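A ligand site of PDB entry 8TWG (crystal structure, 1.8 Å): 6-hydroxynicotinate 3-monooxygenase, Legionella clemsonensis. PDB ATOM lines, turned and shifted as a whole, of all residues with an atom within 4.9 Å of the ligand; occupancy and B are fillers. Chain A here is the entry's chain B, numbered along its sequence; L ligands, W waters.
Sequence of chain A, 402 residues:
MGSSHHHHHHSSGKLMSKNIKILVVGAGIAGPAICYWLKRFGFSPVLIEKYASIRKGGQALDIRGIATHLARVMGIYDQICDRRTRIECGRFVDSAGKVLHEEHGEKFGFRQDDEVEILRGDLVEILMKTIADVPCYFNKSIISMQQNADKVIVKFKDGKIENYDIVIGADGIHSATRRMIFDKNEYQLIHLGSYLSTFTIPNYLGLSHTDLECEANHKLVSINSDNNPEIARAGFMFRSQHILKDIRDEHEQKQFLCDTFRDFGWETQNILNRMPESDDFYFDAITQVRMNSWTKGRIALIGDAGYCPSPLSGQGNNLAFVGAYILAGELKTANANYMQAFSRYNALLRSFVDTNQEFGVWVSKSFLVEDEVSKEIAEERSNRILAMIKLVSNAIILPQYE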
ATOM      1  N   VAL A  25      21.257  17.236  13.805  1.00  0.00           N
ATOM      2  CA  VAL A  25      20.149  18.161  13.646  1.00  0.00           C
ATOM      3  C   VAL A  25      20.050  19.058  14.882  1.00  0.00           C
ATOM      4  O   VAL A  25      19.600  18.608  15.949  1.00  0.00           O
ATOM      5  CB  VAL A  25      18.825  17.419  13.414  1.00  0.00           C
ATOM      6  CG1 VAL A  25      17.695  18.394  13.122  1.00  0.00           C
ATOM      7  CG2 VAL A  25      18.967  16.364  12.304  1.00  0.00           C
ATOM      8  N   GLY A  26      20.396  20.331  14.713  1.00  0.00           N
ATOM      9  CA  GLY A  26      20.253  21.316  15.771  1.00  0.00           C
ATOM     10  C   GLY A  26      21.543  21.930  16.268  1.00  0.00           C
ATOM     11  O   GLY A  26      22.397  21.226  16.806  1.00  0.00           O
ATOM     12  N   ALA A  27      21.704  23.236  16.059  1.00  0.00           N
ATOM     13  CA  ALA A  27      22.916  23.956  16.481  1.00  0.00           C
ATOM     14  C   ALA A  27      22.659  24.732  17.777  1.00  0.00           C
ATOM     15  O   ALA A  27      22.721  25.961  17.824  1.00  0.00           O
ATOM     16  CB  ALA A  27      23.396  24.873  15.360  1.00  0.00           C
ATOM     17  N   GLY A  28      22.365  23.983  18.848  1.00  0.00           N
ATOM     18  CA  GLY A  28      22.242  24.572  20.164  1.00  0.00           C
ATOM     19  C   GLY A  28      23.500  24.346  21.007  1.00  0.00           C
ATOM     20  O   GLY A  28      24.558  24.913  20.748  1.00  0.00           O
ATOM     21  N   ILE A  29      23.382  23.523  22.038  1.00  0.00           N
ATOM     22  CA  ILE A  29      24.520  23.119  22.836  1.00  0.00           C
ATOM     23  C   ILE A  29      24.951  21.695  22.525  1.00  0.00           C
ATOM     24  O   ILE A  29      26.125  21.419  22.265  1.00  0.00           O
ATOM     25  CB  ILE A  29      24.221  23.312  24.342  1.00  0.00           C
ATOM     26  CG1 ILE A  29      24.097  24.824  24.621  1.00  0.00           C
ATOM     27  CG2 ILE A  29      25.283  22.630  25.189  1.00  0.00           C
ATOM     28  CD1 ILE A  29      23.508  25.137  25.939  1.00  0.00           C
ATOM     29  N   ALA A  30      23.993  20.755  22.540  1.00  0.00           N
ATOM     30  CA  ALA A  30      24.325  19.350  22.327  1.00  0.00           C
ATOM     31  C   ALA A  30      24.867  19.087  20.921  1.00  0.00           C
ATOM     32  O   ALA A  30      25.806  18.305  20.760  1.00  0.00           O
ATOM     33  CB  ALA A  30      23.083  18.483  22.584  1.00  0.00           C
ATOM     34  N   GLY A  31      24.268  19.714  19.902  1.00  0.00           N
ATOM     35  CA  GLY A  31      24.610  19.422  18.534  1.00  0.00           C
ATOM     36  C   GLY A  31      26.024  19.869  18.214  1.00  0.00           C
ATOM     37  O   GLY A  31      26.850  19.089  17.724  1.00  0.00           O
ATOM     38  N   ILE A  48      23.084  20.822  10.810  1.00  0.00           N
ATOM     39  CA  ILE A  48      22.051  21.694  10.260  1.00  0.00           C
ATOM     40  C   ILE A  48      21.298  22.403  11.380  1.00  0.00           C
ATOM     41  O   ILE A  48      21.196  21.905  12.516  1.00  0.00           O
ATOM     42  CB  ILE A  48      21.068  20.928   9.348  1.00  0.00           C
ATOM     43  CG1 ILE A  48      20.295  19.859  10.124  1.00  0.00           C
ATOM     44  CG2 ILE A  48      21.819  20.290   8.199  1.00  0.00           C
ATOM     45  CD1 ILE A  48      19.188  19.177   9.330  1.00  0.00           C
ATOM     46  N   GLU A  49      20.765  23.586  11.051  1.00  0.00           N
ATOM     47  CA  GLU A  49      19.976  24.419  11.939  1.00  0.00           C
ATOM     48  C   GLU A  49      18.738  24.909  11.202  1.00  0.00           C
ATOM     49  O   GLU A  49      18.829  25.412  10.085  1.00  0.00           O
ATOM     50  CB  GLU A  49      20.818  25.593  12.440  1.00  0.00           C
ATOM     51  CG  GLU A  49      20.056  26.675  13.190  1.00  0.00           C
ATOM     52  CD  GLU A  49      19.334  26.145  14.401  1.00  0.00           C
ATOM     53  OE1 GLU A  49      19.909  25.286  15.112  1.00  0.00           O
ATOM     54  OE2 GLU A  49      18.174  26.561  14.629  1.00  0.00           O
ATOM     55  N   LYS A  50      17.581  24.767  11.836  1.00  0.00           N
ATOM     56  CA  LYS A  50      16.329  25.211  11.227  1.00  0.00           C
ATOM     57  C   LYS A  50      16.313  26.720  11.043  1.00  0.00           C
ATOM     58  O   LYS A  50      15.824  27.213  10.025  1.00  0.00           O
ATOM     59  CB  LYS A  50      15.143  24.769  12.109  1.00  0.00           C
ATOM     60  CG  LYS A  50      13.797  25.415  11.749  1.00  0.00           C
ATOM     61  CD  LYS A  50      12.830  25.387  12.927  1.00  0.00           C
ATOM     62  CE  LYS A  50      12.215  24.014  13.137  1.00  0.00           C
ATOM     63  NZ  LYS A  50      11.323  23.980  14.346  1.00  0.00           N
ATOM     64  N   TYR A  51      16.789  27.471  12.026  1.00  0.00           N
ATOM     65  CA  TYR A  51      16.757  28.923  11.930  1.00  0.00           C
ATOM     66  C   TYR A  51      17.825  29.430  10.959  1.00  0.00           C
ATOM     67  O   TYR A  51      18.719  28.699  10.537  1.00  0.00           O
ATOM     68  CB  TYR A  51      16.967  29.551  13.301  1.00  0.00           C
ATOM     69  CG  TYR A  51      15.720  29.581  14.132  1.00  0.00           C
ATOM     70  CD1 TYR A  51      15.173  28.410  14.645  1.00  0.00           C
ATOM     71  CD2 TYR A  51      15.077  30.780  14.397  1.00  0.00           C
ATOM     72  CE1 TYR A  51      14.025  28.435  15.405  1.00  0.00           C
ATOM     73  CE2 TYR A  51      13.928  30.810  15.165  1.00  0.00           C
ATOM     74  CZ  TYR A  51      13.409  29.645  15.665  1.00  0.00           C
ATOM     75  OH  TYR A  51      12.270  29.674  16.422  1.00  0.00           O
ATOM     76  N   ARG A  55      21.059  30.844  17.276  1.00  0.00           N
ATOM     77  CA  ARG A  55      20.197  31.494  18.263  1.00  0.00           C
ATOM     78  C   ARG A  55      20.976  31.717  19.550  1.00  0.00           C
ATOM     79  O   ARG A  55      21.426  30.750  20.166  1.00  0.00           O
ATOM     80  CB  ARG A  55      18.965  30.631  18.518  1.00  0.00           C
ATOM     81  CG  ARG A  55      18.239  30.180  17.248  1.00  0.00           C
ATOM     82  CD  ARG A  55      17.229  29.085  17.542  1.00  0.00           C
ATOM     83  NE  ARG A  55      16.139  29.545  18.405  1.00  0.00           N
ATOM     84  CZ  ARG A  55      15.164  28.751  18.854  1.00  0.00           C
ATOM     85  NH1 ARG A  55      15.135  27.470  18.562  1.00  0.00           N
ATOM     86  NH2 ARG A  55      14.211  29.264  19.625  1.00  0.00           N
ATOM     87  N   GLY A  57      19.880  33.718  22.313  1.00  0.00           N
ATOM     88  CA  GLY A  57      19.108  34.068  23.485  1.00  0.00           C
ATOM     89  C   GLY A  57      19.345  33.085  24.603  1.00  0.00           C
ATOM     90  O   GLY A  57      20.104  32.118  24.479  1.00  0.00           O
ATOM     91  N   GLY A  58      18.682  33.338  25.733  1.00  0.00           N
ATOM     92  CA  GLY A  58      18.753  32.452  26.880  1.00  0.00           C
ATOM     93  C   GLY A  58      19.381  33.095  28.105  1.00  0.00           C
ATOM     94  O   GLY A  58      20.191  34.020  28.021  1.00  0.00           O
ATOM     95  N   GLN A  59      18.999  32.579  29.282  1.00  0.00           N
ATOM     96  CA  GLN A  59      19.542  33.065  30.532  1.00  0.00           C
ATOM     97  C   GLN A  59      20.983  32.570  30.721  1.00  0.00           C
ATOM     98  O   GLN A  59      21.499  31.796  29.911  1.00  0.00           O
ATOM     99  CB  GLN A  59      18.710  32.557  31.725  1.00  0.00           C
ATOM    100  CG  GLN A  59      17.259  33.042  31.702  1.00  0.00           C
ATOM    101  CD  GLN A  59      16.558  32.859  33.029  1.00  0.00           C
ATOM    102  OE1 GLN A  59      16.567  31.752  33.619  1.00  0.00           O
ATOM    103  NE2 GLN A  59      15.947  33.913  33.515  1.00  0.00           N
ATOM    104  N   ARG A 120      23.993  31.733  27.986  1.00  0.00           N
ATOM    105  CA  ARG A 120      23.857  30.683  26.996  1.00  0.00           C
ATOM    106  C   ARG A 120      24.416  31.097  25.645  1.00  0.00           C
ATOM    107  O   ARG A 120      25.128  30.337  24.988  1.00  0.00           O
ATOM    108  CB  ARG A 120      22.378  30.295  26.831  1.00  0.00           C
ATOM    109  CG  ARG A 120      22.182  29.184  25.790  1.00  0.00           C
ATOM    110  CD  ARG A 120      20.687  28.858  25.613  1.00  0.00           C
ATOM    111  NE  ARG A 120      20.520  27.804  24.623  1.00  0.00           N
ATOM    112  CZ  ARG A 120      20.650  27.974  23.317  1.00  0.00           C
ATOM    113  NH1 ARG A 120      20.844  29.172  22.791  1.00  0.00           N
ATOM    114  NH2 ARG A 120      20.547  26.923  22.512  1.00  0.00           N
ATOM    115  N   LYS A 140      17.782  24.938   7.040  1.00  0.00           N
ATOM    116  CA  LYS A 140      17.514  23.569   6.612  1.00  0.00           C
ATOM    117  C   LYS A 140      16.541  22.947   7.608  1.00  0.00           C
ATOM    118  O   LYS A 140      16.811  22.906   8.806  1.00  0.00           O
ATOM    119  CB  LYS A 140      18.801  22.750   6.538  1.00  0.00           C
ATOM    120  CG  LYS A 140      19.594  22.939   5.247  1.00  0.00           C
ATOM    121  CD  LYS A 140      18.825  22.480   4.025  1.00  0.00           C
ATOM    122  CE  LYS A 140      19.746  22.164   2.843  1.00  0.00           C
ATOM    123  NZ  LYS A 140      20.438  20.843   3.017  1.00  0.00           N
ATOM    124  N   SER A 141      15.415  22.459   7.094  1.00  0.00           N
ATOM    125  CA  SER A 141      14.369  21.898   7.936  1.00  0.00           C
ATOM    126  C   SER A 141      13.868  20.616   7.320  1.00  0.00           C
ATOM    127  O   SER A 141      13.466  20.597   6.158  1.00  0.00           O
ATOM    128  CB  SER A 141      13.216  22.888   8.117  1.00  0.00           C
ATOM    129  OG  SER A 141      12.293  22.427   9.083  1.00  0.00           O
ATOM    130  N   ALA A 170      19.593  16.510  17.819  1.00  0.00           N
ATOM    131  CA  ALA A 170      20.039  17.453  18.830  1.00  0.00           C
ATOM    132  C   ALA A 170      19.146  18.685  18.810  1.00  0.00           C
ATOM    133  O   ALA A 170      19.599  19.810  19.029  1.00  0.00           O
ATOM    134  CB  ALA A 170      21.503  17.822  18.614  1.00  0.00           C
ATOM    135  N   ASP A 171      17.853  18.482  18.516  1.00  0.00           N
ATOM    136  CA  ASP A 171      16.970  19.588  18.188  1.00  0.00           C
ATOM    137  C   ASP A 171      16.021  19.960  19.338  1.00  0.00           C
ATOM    138  O   ASP A 171      14.940  20.539  19.087  1.00  0.00           O
ATOM    139  CB  ASP A 171      16.200  19.286  16.889  1.00  0.00           C
ATOM    140  CG  ASP A 171      15.717  17.832  16.784  1.00  0.00           C
ATOM    141  OD1 ASP A 171      15.994  16.995  17.662  1.00  0.00           O
ATOM    142  OD2 ASP A 171      15.011  17.528  15.789  1.00  0.00           O
ATOM    143  N   GLY A 172      16.424  19.718  20.577  1.00  0.00           N
ATOM    144  CA  GLY A 172      15.754  20.336  21.707  1.00  0.00           C
ATOM    145  C   GLY A 172      14.518  19.594  22.169  1.00  0.00           C
ATOM    146  O   GLY A 172      14.115  18.568  21.644  1.00  0.00           O
ATOM    147  N   ILE A 173      13.860  20.185  23.178  1.00  0.00           N
ATOM    148  CA  ILE A 173      12.760  19.490  23.840  1.00  0.00           C
ATOM    149  C   ILE A 173      11.618  19.195  22.872  1.00  0.00           C
ATOM    150  O   ILE A 173      10.891  18.215  23.050  1.00  0.00           O
ATOM    151  CB  ILE A 173      12.240  20.290  25.061  1.00  0.00           C
ATOM    152  CG1 ILE A 173      11.098  19.510  25.722  1.00  0.00           C
ATOM    153  CG2 ILE A 173      11.802  21.679  24.632  1.00  0.00           C
ATOM    154  CD1 ILE A 173      11.059  19.621  27.208  1.00  0.00           C
ATOM    155  N   ALA A 176      11.832  17.563  16.415  1.00  0.00           N
ATOM    156  CA  ALA A 176      11.161  16.996  15.248  1.00  0.00           C
ATOM    157  C   ALA A 176      11.706  15.615  14.931  1.00  0.00           C
ATOM    158  O   ALA A 176      10.955  14.714  14.533  1.00  0.00           O
ATOM    159  CB  ALA A 176      11.345  17.933  14.053  1.00  0.00           C
ATOM    160  N   LEU A 196       8.932  29.463  31.656  1.00  0.00           N
ATOM    161  CA  LEU A 196      10.089  30.351  31.659  1.00  0.00           C
ATOM    162  C   LEU A 196      10.079  31.205  30.407  1.00  0.00           C
ATOM    163  O   LEU A 196       9.831  30.700  29.298  1.00  0.00           O
ATOM    164  CB  LEU A 196      11.408  29.535  31.711  1.00  0.00           C
ATOM    165  CG  LEU A 196      12.687  30.290  31.405  1.00  0.00           C
ATOM    166  CD1 LEU A 196      12.907  31.442  32.366  1.00  0.00           C
ATOM    167  CD2 LEU A 196      13.817  29.284  31.496  1.00  0.00           C
ATOM    168  N   THR A 198      12.583  34.548  28.645  1.00  0.00           N
ATOM    169  CA  THR A 198      13.709  35.466  28.789  1.00  0.00           C
ATOM    170  C   THR A 198      13.985  36.146  27.446  1.00  0.00           C
ATOM    171  O   THR A 198      13.782  35.569  26.369  1.00  0.00           O
ATOM    172  CB  THR A 198      14.988  34.769  29.335  1.00  0.00           C
ATOM    173  OG1 THR A 198      16.014  35.769  29.532  1.00  0.00           O
ATOM    174  CG2 THR A 198      15.513  33.704  28.391  1.00  0.00           C
ATOM    175  N   ARG A 248       4.333  26.373  20.091  1.00  0.00           N
ATOM    176  CA  ARG A 248       5.298  27.049  19.237  1.00  0.00           C
ATOM    177  C   ARG A 248       4.816  28.403  18.723  1.00  0.00           C
ATOM    178  O   ARG A 248       5.592  29.123  18.086  1.00  0.00           O
ATOM    179  CB  ARG A 248       5.646  26.168  18.029  1.00  0.00           C
ATOM    180  CG  ARG A 248       5.900  24.700  18.354  1.00  0.00           C
ATOM    181  CD  ARG A 248       7.075  24.510  19.309  1.00  0.00           C
ATOM    182  NE  ARG A 248       8.379  24.787  18.711  1.00  0.00           N
ATOM    183  CZ  ARG A 248       8.993  23.993  17.848  1.00  0.00           C
ATOM    184  NH1 ARG A 248       8.430  22.879  17.398  1.00  0.00           N
ATOM    185  NH2 ARG A 248      10.223  24.308  17.419  1.00  0.00           N
ATOM    186  N   TYR A 282      12.594  34.175  23.995  1.00  0.00           N
ATOM    187  CA  TYR A 282      12.531  32.763  24.327  1.00  0.00           C
ATOM    188  C   TYR A 282      11.395  32.534  25.310  1.00  0.00           C
ATOM    189  O   TYR A 282      11.235  33.282  26.282  1.00  0.00           O
ATOM    190  CB  TYR A 282      13.854  32.280  24.938  1.00  0.00           C
ATOM    191  CG  TYR A 282      13.804  30.839  25.402  1.00  0.00           C
ATOM    192  CD1 TYR A 282      13.906  29.803  24.487  1.00  0.00           C
ATOM    193  CD2 TYR A 282      13.669  30.533  26.739  1.00  0.00           C
ATOM    194  CE1 TYR A 282      13.889  28.495  24.889  1.00  0.00           C
ATOM    195  CE2 TYR A 282      13.615  29.191  27.159  1.00  0.00           C
ATOM    196  CZ  TYR A 282      13.751  28.191  26.213  1.00  0.00           C
ATOM    197  OH  TYR A 282      13.719  26.871  26.564  1.00  0.00           O
ATOM    198  N   ILE A 302      20.193  13.201  21.452  1.00  0.00           N
ATOM    199  CA  ILE A 302      21.064  13.716  22.510  1.00  0.00           C
ATOM    200  C   ILE A 302      20.454  14.973  23.100  1.00  0.00           C
ATOM    201  O   ILE A 302      19.632  15.644  22.480  1.00  0.00           O
ATOM    202  CB  ILE A 302      22.491  13.999  22.007  1.00  0.00           C
ATOM    203  CG1 ILE A 302      22.501  15.056  20.907  1.00  0.00           C
ATOM    204  CG2 ILE A 302      23.159  12.684  21.545  1.00  0.00           C
ATOM    205  CD1 ILE A 302      23.925  15.529  20.515  1.00  0.00           C
ATOM    206  N   GLY A 303      20.898  15.311  24.315  1.00  0.00           N
ATOM    207  CA  GLY A 303      20.450  16.539  24.953  1.00  0.00           C
ATOM    208  C   GLY A 303      18.965  16.546  25.244  1.00  0.00           C
ATOM    209  O   GLY A 303      18.370  15.497  25.513  1.00  0.00           O
ATOM    210  N   ASP A 304      18.370  17.736  25.194  1.00  0.00           N
ATOM    211  CA  ASP A 304      16.974  17.894  25.600  1.00  0.00           C
ATOM    212  C   ASP A 304      16.046  17.028  24.771  1.00  0.00           C
ATOM    213  O   ASP A 304      15.023  16.565  25.283  1.00  0.00           O
ATOM    214  CB  ASP A 304      16.546  19.359  25.463  1.00  0.00           C
ATOM    215  CG  ASP A 304      16.861  20.187  26.715  1.00  0.00           C
ATOM    216  OD1 ASP A 304      17.508  19.680  27.658  1.00  0.00           O
ATOM    217  OD2 ASP A 304      16.434  21.353  26.758  1.00  0.00           O
ATOM    218  N   ALA A 305      16.404  16.766  23.503  1.00  0.00           N
ATOM    219  CA  ALA A 305      15.584  15.962  22.621  1.00  0.00           C
ATOM    220  C   ALA A 305      15.261  14.606  23.229  1.00  0.00           C
ATOM    221  O   ALA A 305      14.171  14.064  23.046  1.00  0.00           O
ATOM    222  CB  ALA A 305      16.285  15.762  21.269  1.00  0.00           C
ATOM    223  N   PRO A 311      14.614  23.477  32.950  1.00  0.00           N
ATOM    224  CA  PRO A 311      15.380  24.570  33.573  1.00  0.00           C
ATOM    225  C   PRO A 311      15.502  24.458  35.080  1.00  0.00           C
ATOM    226  O   PRO A 311      16.478  24.953  35.627  1.00  0.00           O
ATOM    227  CB  PRO A 311      14.580  25.820  33.180  1.00  0.00           C
ATOM    228  CG  PRO A 311      13.866  25.462  31.951  1.00  0.00           C
ATOM    229  CD  PRO A 311      13.577  23.982  32.020  1.00  0.00           C
ATOM    230  N   GLY A 316      20.510  21.158  32.226  1.00  0.00           N
ATOM    231  CA  GLY A 316      20.304  20.755  30.844  1.00  0.00           C
ATOM    232  C   GLY A 316      21.588  20.818  30.009  1.00  0.00           C
ATOM    233  O   GLY A 316      21.894  19.904  29.231  1.00  0.00           O
ATOM    234  N   ASN A 317      22.341  21.896  30.145  1.00  0.00           N
ATOM    235  CA  ASN A 317      23.542  22.065  29.326  1.00  0.00           C
ATOM    236  C   ASN A 317      24.632  21.072  29.729  1.00  0.00           C
ATOM    237  O   ASN A 317      25.426  20.650  28.886  1.00  0.00           O
ATOM    238  CB  ASN A 317      24.046  23.499  29.443  1.00  0.00           C
ATOM    239  CG  ASN A 317      24.245  23.940  30.873  1.00  0.00           C
ATOM    240  OD1 ASN A 317      23.260  24.197  31.602  1.00  0.00           O
ATOM    241  ND2 ASN A 317      25.497  24.086  31.299  1.00  0.00           N
ATOM    242  N   ALA A 320      23.662  17.773  28.326  1.00  0.00           N
ATOM    243  CA  ALA A 320      23.969  17.809  26.898  1.00  0.00           C
ATOM    244  C   ALA A 320      25.455  17.552  26.656  1.00  0.00           C
ATOM    245  O   ALA A 320      25.811  16.762  25.766  1.00  0.00           O
ATOM    246  CB  ALA A 320      23.537  19.147  26.315  1.00  0.00           C
HETATM  247  P1  LIG L   1      18.519  23.455  22.557  1.00  0.00           P
HETATM  248  O1  LIG L   1      19.417  24.330  23.299  1.00  0.00           O
HETATM  249  O2  LIG L   1      17.011  23.705  22.720  1.00  0.00           O
HETATM  250  O3  LIG L   1      18.957  23.504  21.037  1.00  0.00           O
HETATM  251  C1  LIG L   1      18.129  22.920  19.997  1.00  0.00           C
HETATM  252  C2  LIG L   1      18.599  23.477  18.665  1.00  0.00           C
HETATM  253  O4  LIG L   1      17.968  22.741  17.584  1.00  0.00           O
HETATM  254  C3  LIG L   1      18.248  24.958  18.443  1.00  0.00           C
HETATM  255  O5  LIG L   1      19.361  25.620  17.846  1.00  0.00           O
HETATM  256  C4  LIG L   1      17.006  24.884  17.551  1.00  0.00           C
HETATM  257  O6  LIG L   1      16.811  26.018  16.718  1.00  0.00           O
HETATM  258  C5  LIG L   1      17.357  23.667  16.694  1.00  0.00           C
HETATM  259  N1  LIG L   1      16.209  23.025  16.071  1.00  0.00           N
HETATM  260  C6  LIG L   1      14.953  22.863  16.585  1.00  0.00           C
HETATM  261  N2  LIG L   1      14.134  22.222  15.784  1.00  0.00           N
HETATM  262  C7  LIG L   1      14.912  21.935  14.669  1.00  0.00           C
HETATM  263  C8  LIG L   1      14.623  21.275  13.461  1.00  0.00           C
HETATM  264  N3  LIG L   1      13.428  20.754  13.169  1.00  0.00           N
HETATM  265  N4  LIG L   1      15.622  21.154  12.564  1.00  0.00           N
HETATM  266  C9  LIG L   1      16.821  21.662  12.852  1.00  0.00           C
HETATM  267  N5  LIG L   1      17.199  22.326  13.947  1.00  0.00           N
HETATM  268  C10 LIG L   1      16.187  22.422  14.835  1.00  0.00           C
HETATM  269  N6  LIG L   1      17.084  26.559  28.931  1.00  0.00           N
HETATM  270  C11 LIG L   1      17.083  27.114  30.170  1.00  0.00           C
HETATM  271  O7  LIG L   1      17.079  26.412  31.197  1.00  0.00           O
HETATM  272  N7  LIG L   1      17.078  28.492  30.313  1.00  0.00           N
HETATM  273  C12 LIG L   1      17.096  29.418  29.264  1.00  0.00           C
HETATM  274  O8  LIG L   1      17.104  30.625  29.515  1.00  0.00           O
HETATM  275  C13 LIG L   1      17.125  28.813  27.940  1.00  0.00           C
HETATM  276  N8  LIG L   1      17.137  29.615  26.880  1.00  0.00           N
HETATM  277  C14 LIG L   1      17.148  29.000  25.618  1.00  0.00           C
HETATM  278  C15 LIG L   1      17.187  29.810  24.486  1.00  0.00           C
HETATM  279  C16 LIG L   1      17.218  29.247  23.208  1.00  0.00           C
HETATM  280  C17 LIG L   1      17.206  30.150  21.998  1.00  0.00           C
HETATM  281  C18 LIG L   1      17.192  27.860  23.057  1.00  0.00           C
HETATM  282  C19 LIG L   1      17.209  27.211  21.688  1.00  0.00           C
HETATM  283  C20 LIG L   1      17.188  27.045  24.193  1.00  0.00           C
HETATM  284  C21 LIG L   1      17.157  27.608  25.472  1.00  0.00           C
HETATM  285  N9  LIG L   1      17.116  26.812  26.630  1.00  0.00           N
HETATM  286  C22 LIG L   1      17.123  27.376  27.876  1.00  0.00           C
HETATM  287  C23 LIG L   1      17.227  25.359  26.547  1.00  0.00           C
HETATM  288  C24 LIG L   1      18.690  24.900  26.820  1.00  0.00           C
HETATM  289  O9  LIG L   1      19.578  25.334  25.776  1.00  0.00           O
HETATM  290  C25 LIG L   1      18.762  23.379  26.980  1.00  0.00           C
HETATM  291  O10 LIG L   1      18.002  23.030  28.144  1.00  0.00           O
HETATM  292  C26 LIG L   1      20.147  22.771  27.091  1.00  0.00           C
HETATM  293  O11 LIG L   1      21.084  23.660  27.713  1.00  0.00           O
HETATM  294  C27 LIG L   1      20.757  22.466  25.724  1.00  0.00           C
HETATM  295  O12 LIG L   1      19.988  21.434  25.100  1.00  0.00           O
HETATM  296  P2  LIG L   1      20.051  21.161  23.557  1.00  0.00           P
HETATM  297  O13 LIG L   1      21.284  21.617  22.784  1.00  0.00           O
HETATM  298  O14 LIG L   1      19.768  19.740  23.548  1.00  0.00           O
HETATM  299  O15 LIG L   1      18.744  21.938  22.976  1.00  0.00           O
HETATM  300  O   HOH W   1      11.508  19.992  10.972  1.00  0.00           O
HETATM  301  O   HOH W   2      20.316  24.147  30.359  1.00  0.00           O
HETATM  302  O   HOH W   3      20.598  27.691  19.646  1.00  0.00           O
HETATM  303  O   HOH W   4      15.331  22.407  24.539  1.00  0.00           O
HETATM  304  O   HOH W   5      20.962  27.908  16.523  1.00  0.00           O
HETATM  305  O   HOH W   6      21.802  21.267  20.093  1.00  0.00           O
HETATM  306  O   HOH W   7      12.476  20.559  16.925  1.00  0.00           O
HETATM  307  O   HOH W   8      20.005  29.463  29.542  1.00  0.00           O
HETATM  308  O   HOH W   9      18.663  18.131  21.897  1.00  0.00           O
HETATM  309  O   HOH W  10      14.535  24.216  21.590  1.00  0.00           O
HETATM  310  O   HOH W  11      14.135  25.230  19.422  1.00  0.00           O
HETATM  311  O   HOH W  12      16.895  21.178  30.503  1.00  0.00           O
HETATM  312  O   HOH W  13      19.697  28.660  32.229  1.00  0.00           O
HETATM  313  O   HOH W  14      17.224  29.321  32.980  1.00  0.00           O
HETATM  314  O   HOH W  15      17.383  24.042  30.688  1.00  0.00           O
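The guanidinium group (NH1) of Arg 120 is in hydrogen-bond range of the backbone carbonyl oxygen (O) of Arg 55, at 3.1 Å.
O of Val 25 sits at hydrogen-bond distance from N of Ala 170 (2.8 Å).
N of Ala 305 sits close to O of Gly 172 (3.5 Å).
The backbone carbonyl oxygen (O) of Glu 49 lies within hydrogen-bond range of the backbone NH (N) of Lys 140, at 3.3 Å.
The side-chain carboxylate of Asp 171 lies within hydrogen-bond range of the backbone NH of Ala 176 (3.2 Å).
The backbone NH (N) of Ala 27 is in hydrogen-bond range of the side-chain carboxylate (OE1) of Glu 49, at 2.9 Å.
The backbone carbonyl oxygen (O) of Thr 198 sits at hydrogen-bond distance from the backbone NH (N) of Tyr 282 (3.0 Å).
The backbone carbonyl oxygen of Gln 59 sits at hydrogen-bond distance from the backbone NH of Arg 120, 3.2 Å away.
N of Ile 29 is in hydrogen-bond range of O13 of the ligand (2.9 Å).
N of Asn 317 is in hydrogen-bond range of O11 of the ligand.
OD2 of Asp 304 is in hydrogen-bond range of O10 of the ligand, 2.7 Å away.
The guanidinium group of Arg 55 is in hydrogen-bond range of an oxygen (O6) of the ligand, 2.9 Å away.
The backbone NH of Asp 304 sits at hydrogen-bond distance from an oxygen (O14) of the ligand (2.9 Å).
NH2 of Arg 120 lies within salt-bridge range of O1 of the ligand (2.9 Å).
O8 of the ligand lies within hydrogen-bond range of N of Gln 59 (2.7 Å).
O5 of the ligand lies within hydrogen-bond range of O of Ala 27 (3.4 Å).
O6 of the ligand is in hydrogen-bond range of OE2 of Glu 49.
N5 of the ligand sits at hydrogen-bond distance from N of Lys 50, 3.2 Å away.
N of Ala 30 lies within hydrogen-bond range of O13 of the ligand (2.9 Å).
OH of Tyr 282 lies close to N9 of the ligand (3.4 Å).
Residues that only touch the ligand: Val 25, Gly 26, Gly 28, Tyr 51, Gly 57, Gly 58, Ala 170, Asp 171, Gly 172, Ala 176, Leu 196, Thr 198, Gly 303, Pro 311 and Gly 316.
Hydrophobic or aromatic side chains that line the ligand: Val 25, Ile 29, Ala 30, Tyr 51, Ala 176, Leu 196, Tyr 282 and Pro 311.
The nearest printed residue that does not touch the ligand is Lys 140 (4.2 Å).
Water W7 lies within hydrogen-bond range of a nitrogen (N2) of the ligand (2.6 Å), the backbone NH of Ala 176 (3.1 Å) and the backbone carbonyl oxygen of Asp 171 (3.3 Å).
Water W14 lies within hydrogen-bond range of OE1 of Gln 59 (2.6 Å) and N7 of the ligand (2.8 Å).
Water W2 lies within hydrogen-bond range of O11 of the ligand (2.8 Å) and N of Asn 317 (3.0 Å).
Water W8 bridges the backbone carbonyl oxygen (O) of Gln 59 (2.8 Å) and an oxygen (O8) of the ligand (3.1 Å).
Water W3 lies within hydrogen-bond range of the guanidinium group (NH2) of Arg 120 (3.0 Å), an oxygen (O5) of the ligand (3.0 Å), the backbone carbonyl oxygen (O) of Arg 55 (3.2 Å) and the backbone carbonyl oxygen (O) of Ala 27 (3.3 Å).
Water W12 bridges an oxygen (O10) of the ligand (3.2 Å) and the side-chain carboxylate (OD1) of Asp 304 (3.3 Å).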
